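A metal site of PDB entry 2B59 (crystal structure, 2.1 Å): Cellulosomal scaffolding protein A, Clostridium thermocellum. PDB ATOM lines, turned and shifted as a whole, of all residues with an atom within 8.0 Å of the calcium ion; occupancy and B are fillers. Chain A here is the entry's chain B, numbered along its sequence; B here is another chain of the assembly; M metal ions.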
ATOM      1  N   VAL A 117     -11.052  -2.042   6.758  1.00  0.00           N
ATOM      2  CA  VAL A 117      -9.892  -1.248   6.384  1.00  0.00           C
ATOM      3  C   VAL A 117      -8.799  -2.196   5.905  1.00  0.00           C
ATOM      4  O   VAL A 117      -8.090  -1.899   4.932  1.00  0.00           O
ATOM      5  CB  VAL A 117      -9.358  -0.433   7.586  1.00  0.00           C
ATOM      6  CG1 VAL A 117      -8.142   0.386   7.159  1.00  0.00           C
ATOM      7  CG2 VAL A 117     -10.445   0.477   8.126  1.00  0.00           C
ATOM      8  N   ALA A 123      -3.452   0.045   0.026  1.00  0.00           N
ATOM      9  CA  ALA A 123      -3.958   0.631  -1.211  1.00  0.00           C
ATOM     10  C   ALA A 123      -3.550   2.106  -1.263  1.00  0.00           C
ATOM     11  O   ALA A 123      -3.514   2.781  -0.238  1.00  0.00           O
ATOM     12  CB  ALA A 123      -5.478   0.507  -1.271  1.00  0.00           C
ATOM     13  N   TYR A 130      -8.339   1.128  -3.650  1.00  0.00           N
ATOM     14  CA  TYR A 130      -8.404   2.312  -2.802  1.00  0.00           C
ATOM     15  C   TYR A 130      -9.817   2.893  -2.710  1.00  0.00           C
ATOM     16  O   TYR A 130     -10.488   3.079  -3.727  1.00  0.00           O
ATOM     17  CB  TYR A 130      -7.434   3.380  -3.313  1.00  0.00           C
ATOM     18  CG  TYR A 130      -7.436   4.656  -2.494  1.00  0.00           C
ATOM     19  CD1 TYR A 130      -8.357   5.669  -2.755  1.00  0.00           C
ATOM     20  CD2 TYR A 130      -6.489   4.857  -1.483  1.00  0.00           C
ATOM     21  CE1 TYR A 130      -8.361   6.851  -2.013  1.00  0.00           C
ATOM     22  CE2 TYR A 130      -6.480   6.032  -0.732  1.00  0.00           C
ATOM     23  CZ  TYR A 130      -7.416   7.029  -0.997  1.00  0.00           C
ATOM     24  OH  TYR A 130      -7.403   8.197  -0.280  1.00  0.00           O
ATOM     25  N   GLU A 132     -11.538   6.130  -0.764  1.00  0.00           N
ATOM     26  CA  GLU A 132     -11.276   7.324   0.026  1.00  0.00           C
ATOM     27  C   GLU A 132     -11.826   7.296   1.465  1.00  0.00           C
ATOM     28  O   GLU A 132     -11.107   7.677   2.396  1.00  0.00           O
ATOM     29  CB  GLU A 132     -11.786   8.578  -0.702  1.00  0.00           C
ATOM     30  CG  GLU A 132     -11.266   9.878  -0.096  1.00  0.00           C
ATOM     31  CD  GLU A 132     -11.608  11.102  -0.942  1.00  0.00           C
ATOM     32  OE1 GLU A 132     -11.070  12.199  -0.645  1.00  0.00           O
ATOM     33  OE2 GLU A 132     -12.401  10.978  -1.900  1.00  0.00           O
ATOM     34  N   LEU A 134     -12.167   4.947   3.452  1.00  0.00           N
ATOM     35  CA  LEU A 134     -11.396   4.048   4.308  1.00  0.00           C
ATOM     36  C   LEU A 134     -10.005   4.614   4.584  1.00  0.00           C
ATOM     37  O   LEU A 134      -9.287   4.133   5.462  1.00  0.00           O
ATOM     38  CB  LEU A 134     -11.310   2.656   3.667  1.00  0.00           C
ATOM     39  CG  LEU A 134     -12.679   1.996   3.428  1.00  0.00           C
ATOM     40  CD1 LEU A 134     -12.482   0.621   2.819  1.00  0.00           C
ATOM     41  CD2 LEU A 134     -13.446   1.898   4.742  1.00  0.00           C
ATOM     42  N   ASP A 135      -9.637   5.643   3.827  1.00  0.00           N
ATOM     43  CA  ASP A 135      -8.361   6.323   4.017  1.00  0.00           C
ATOM     44  C   ASP A 135      -8.667   7.378   5.085  1.00  0.00           C
ATOM     45  O   ASP A 135      -8.761   8.571   4.788  1.00  0.00           O
ATOM     46  CB  ASP A 135      -7.925   6.983   2.700  1.00  0.00           C
ATOM     47  CG  ASP A 135      -6.691   7.848   2.868  1.00  0.00           C
ATOM     48  OD1 ASP A 135      -6.153   7.888   3.989  1.00  0.00           O
ATOM     49  OD2 ASP A 135      -6.262   8.496   1.889  1.00  0.00           O
ATOM     50  N   ILE A 136      -8.832   6.914   6.321  1.00  0.00           N
ATOM     51  CA  ILE A 136      -9.169   7.738   7.482  1.00  0.00           C
ATOM     52  C   ILE A 136      -8.579   9.139   7.580  1.00  0.00           C
ATOM     53  O   ILE A 136      -9.330  10.101   7.711  1.00  0.00           O
ATOM     54  CB  ILE A 136      -8.862   6.996   8.806  1.00  0.00           C
ATOM     55  CG1 ILE A 136      -9.473   5.591   8.773  1.00  0.00           C
ATOM     56  CG2 ILE A 136      -9.437   7.774   9.989  1.00  0.00           C
ATOM     57  CD1 ILE A 136     -10.989   5.566   8.711  1.00  0.00           C
ATOM     58  N   ASN A 137      -7.255   9.276   7.542  1.00  0.00           N
ATOM     59  CA  ASN A 137      -6.661  10.600   7.648  1.00  0.00           C
ATOM     60  C   ASN A 137      -6.454  11.265   6.278  1.00  0.00           C
ATOM     61  O   ASN A 137      -5.854  12.339   6.184  1.00  0.00           O
ATOM     62  CB  ASN A 137      -5.337  10.554   8.443  1.00  0.00           C
ATOM     63  CG  ASN A 137      -4.234   9.789   7.723  1.00  0.00           C
ATOM     64  OD1 ASN A 137      -4.446   9.257   6.659  1.00  0.00           O
ATOM     65  ND2 ASN A 137      -3.046   9.758   8.330  1.00  0.00           N
ATOM     66  N   ARG A 138      -6.949  10.606   5.233  1.00  0.00           N
ATOM     67  CA  ARG A 138      -6.881  11.133   3.863  1.00  0.00           C
ATOM     68  C   ARG A 138      -5.485  11.528   3.358  1.00  0.00           C
ATOM     69  O   ARG A 138      -5.361  12.496   2.606  1.00  0.00           O
ATOM     70  CB  ARG A 138      -7.789  12.359   3.740  1.00  0.00           C
ATOM     71  CG  ARG A 138      -9.242  12.152   4.168  1.00  0.00           C
ATOM     72  CD  ARG A 138     -10.073  11.500   3.072  1.00  0.00           C
ATOM     73  NE  ARG A 138     -11.455  11.968   3.100  1.00  0.00           N
ATOM     74  CZ  ARG A 138     -12.388  11.499   3.919  1.00  0.00           C
ATOM     75  NH1 ARG A 138     -12.075  10.531   4.772  1.00  0.00           N
ATOM     76  NH2 ARG A 138     -13.615  11.995   3.898  1.00  0.00           N
ATOM     77  N   ASN A 139      -4.448  10.795   3.754  1.00  0.00           N
ATOM     78  CA  ASN A 139      -3.094  11.148   3.300  1.00  0.00           C
ATOM     79  C   ASN A 139      -2.683  10.437   2.006  1.00  0.00           C
ATOM     80  O   ASN A 139      -1.527  10.524   1.589  1.00  0.00           O
ATOM     81  CB  ASN A 139      -2.058  10.879   4.398  1.00  0.00           C
ATOM     82  CG  ASN A 139      -1.855   9.415   4.657  1.00  0.00           C
ATOM     83  OD1 ASN A 139      -2.549   8.573   4.094  1.00  0.00           O
ATOM     84  ND2 ASN A 139      -0.890   9.078   5.525  1.00  0.00           N
ATOM     85  N   GLY A 140      -3.628   9.739   1.367  1.00  0.00           N
ATOM     86  CA  GLY A 140      -3.326   9.070   0.113  1.00  0.00           C
ATOM     87  C   GLY A 140      -3.029   7.576   0.145  1.00  0.00           C
ATOM     88  O   GLY A 140      -2.775   6.981  -0.903  1.00  0.00           O
ATOM     89  N   ALA A 141      -3.059   6.966   1.328  1.00  0.00           N
ATOM     90  CA  ALA A 141      -2.788   5.532   1.428  1.00  0.00           C
ATOM     91  C   ALA A 141      -3.568   4.939   2.581  1.00  0.00           C
ATOM     92  O   ALA A 141      -3.813   5.603   3.558  1.00  0.00           O
ATOM     93  CB  ALA A 141      -1.302   5.296   1.625  1.00  0.00           C
ATOM     94  N   ILE A 142      -3.960   3.677   2.465  1.00  0.00           N
ATOM     95  CA  ILE A 142      -4.691   3.008   3.536  1.00  0.00           C
ATOM     96  C   ILE A 142      -3.695   2.066   4.198  1.00  0.00           C
ATOM     97  O   ILE A 142      -3.187   1.153   3.549  1.00  0.00           O
ATOM     98  CB  ILE A 142      -5.895   2.226   2.977  1.00  0.00           C
ATOM     99  CG1 ILE A 142      -6.884   3.191   2.323  1.00  0.00           C
ATOM    100  CG2 ILE A 142      -6.565   1.431   4.102  1.00  0.00           C
ATOM    101  CD1 ILE A 142      -8.064   2.512   1.628  1.00  0.00           C
ATOM    102  N   ASN A 143      -3.423   2.289   5.476  1.00  0.00           N
ATOM    103  CA  ASN A 143      -2.442   1.463   6.179  1.00  0.00           C
ATOM    104  C   ASN A 143      -2.659   1.390   7.690  1.00  0.00           C
ATOM    105  O   ASN A 143      -3.732   1.743   8.196  1.00  0.00           O
ATOM    106  CB  ASN A 143      -1.035   2.013   5.882  1.00  0.00           C
ATOM    107  CG  ASN A 143      -0.921   3.507   6.145  1.00  0.00           C
ATOM    108  OD1 ASN A 143      -1.529   4.020   7.079  1.00  0.00           O
ATOM    109  ND2 ASN A 143      -0.143   4.202   5.314  1.00  0.00           N
ATOM    110  N   MET A 144      -1.633   0.944   8.419  1.00  0.00           N
ATOM    111  CA  MET A 144      -1.740   0.808   9.870  1.00  0.00           C
ATOM    112  C   MET A 144      -2.044   2.125  10.604  1.00  0.00           C
ATOM    113  O   MET A 144      -2.661   2.110  11.668  1.00  0.00           O
ATOM    114  CB  MET A 144      -0.483   0.167  10.441  1.00  0.00           C
ATOM    115  CG  MET A 144      -0.543  -0.118  11.948  1.00  0.00           C
ATOM    116  SD  MET A 144      -1.884  -1.244  12.451  1.00  0.00           S
ATOM    117  CE  MET A 144      -2.875  -0.199  13.346  1.00  0.00           C
ATOM    118  N   GLN A 145      -1.594   3.245  10.044  1.00  0.00           N
ATOM    119  CA  GLN A 145      -1.846   4.541  10.681  1.00  0.00           C
ATOM    120  C   GLN A 145      -3.365   4.786  10.797  1.00  0.00           C
ATOM    121  O   GLN A 145      -3.836   5.329  11.793  1.00  0.00           O
ATOM    122  CB  GLN A 145      -1.190   5.663   9.857  1.00  0.00           C
ATOM    123  CG  GLN A 145      -1.602   7.070  10.286  1.00  0.00           C
ATOM    124  CD  GLN A 145      -0.785   8.166   9.613  1.00  0.00           C
ATOM    125  OE1 GLN A 145      -0.452   8.063   8.437  1.00  0.00           O
ATOM    126  NE2 GLN A 145      -0.487   9.221  10.356  1.00  0.00           N
ATOM    127  N   ASP A 146      -4.110   4.392   9.766  1.00  0.00           N
ATOM    128  CA  ASP A 146      -5.555   4.567   9.767  1.00  0.00           C
ATOM    129  C   ASP A 146      -6.216   3.622  10.763  1.00  0.00           C
ATOM    130  O   ASP A 146      -7.171   3.988  11.438  1.00  0.00           O
ATOM    131  CB  ASP A 146      -6.132   4.282   8.389  1.00  0.00           C
ATOM    132  CG  ASP A 146      -5.594   5.207   7.344  1.00  0.00           C
ATOM    133  OD1 ASP A 146      -4.915   4.716   6.412  1.00  0.00           O
ATOM    134  OD2 ASP A 146      -5.838   6.424   7.471  1.00  0.00           O
ATOM    135  N   ILE A 147      -5.699   2.403  10.811  1.00  0.00           N
ATOM    136  CA  ILE A 147      -6.225   1.403  11.730  1.00  0.00           C
ATOM    137  C   ILE A 147      -6.026   1.872  13.166  1.00  0.00           C
ATOM    138  O   ILE A 147      -6.914   1.740  13.995  1.00  0.00           O
ATOM    139  CB  ILE A 147      -5.526   0.038  11.493  1.00  0.00           C
ATOM    140  CG1 ILE A 147      -5.894  -0.469  10.095  1.00  0.00           C
ATOM    141  CG2 ILE A 147      -5.947  -0.961  12.552  1.00  0.00           C
ATOM    142  CD1 ILE A 147      -5.182  -1.738   9.687  1.00  0.00           C
ATOM    143  N   ILE A 149      -6.077   4.813  14.293  1.00  0.00           N
ATOM    144  CA  ILE A 149      -7.049   5.863  14.593  1.00  0.00           C
ATOM    145  C   ILE A 149      -8.360   5.199  15.016  1.00  0.00           C
ATOM    146  O   ILE A 149      -9.002   5.620  15.983  1.00  0.00           O
ATOM    147  CB  ILE A 149      -7.297   6.782  13.365  1.00  0.00           C
ATOM    148  CG1 ILE A 149      -6.056   7.641  13.122  1.00  0.00           C
ATOM    149  CG2 ILE A 149      -8.537   7.649  13.591  1.00  0.00           C
ATOM    150  CD1 ILE A 149      -6.100   8.446  11.824  1.00  0.00           C
ATOM    151  N   SER B 151       3.002   3.216  -0.176  1.00  0.00           N
ATOM    152  CA  SER B 151       1.858   2.870   0.664  1.00  0.00           C
ATOM    153  C   SER B 151       2.032   3.307   2.121  1.00  0.00           C
ATOM    154  O   SER B 151       1.168   3.068   2.962  1.00  0.00           O
ATOM    155  CB  SER B 151       1.575   1.367   0.593  1.00  0.00           C
ATOM    156  OG  SER B 151       2.603   0.635   1.212  1.00  0.00           O
ATOM    157  N   PRO B 153       3.169   6.830   3.289  1.00  0.00           N
ATOM    158  CA  PRO B 153       3.618   8.227   3.237  1.00  0.00           C
ATOM    159  C   PRO B 153       3.891   8.820   4.621  1.00  0.00           C
ATOM    160  O   PRO B 153       3.151   8.574   5.570  1.00  0.00           O
ATOM    161  CB  PRO B 153       2.458   8.921   2.506  1.00  0.00           C
ATOM    162  CG  PRO B 153       1.268   8.087   2.879  1.00  0.00           C
ATOM    163  CD  PRO B 153       1.795   6.681   2.775  1.00  0.00           C
HETATM  164 CA    CA M   1      -4.199   7.072   5.465  1.00  0.00          CA
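The calcium ion is bound by O of Ala 141 (2.4 Å), OD1 of Asn 137 (2.5 Å), OD1 of Asp 135 (2.6 Å), OD1 of Asn 139 (2.6 Å), OD1 of Asp 146 (2.6 Å) and OD2 of Asp 146 (2.7 Å).
Within 4 Å of the calcium ion: Asp 135, Asn 137, Asn 139, Ala 141 and Asp 146. The nearest printed residue that does not touch the calcium ion is Asn 143 (4.4 Å).
ND2 of Asn 137 sits close to OE1 of Gln 145 (3.1 Å). N of Arg 138 sits close to OD1 of Asp 135, 3.1 Å away. OD2 of Asp 135 lies within hydrogen-bond range of N of Gly 140, 3.0 Å away. The side-chain hydroxyl of Tyr 130 sits at hydrogen-bond distance from the side-chain carboxylate of Asp 135 (2.5 Å). The side-chain amide oxygen of Gln 145 sits at hydrogen-bond distance from the side-chain amide nitrogen of Asn 139 (3.1 Å). The side-chain carboxylate (OD1) of Asp 146 sits close to the backbone NH (N) of Asn 143 (3.0 Å). The side-chain carboxylate (OD2) of Asp 146 lies close to the backbone NH (N) of Ile 136 (3.2 Å).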
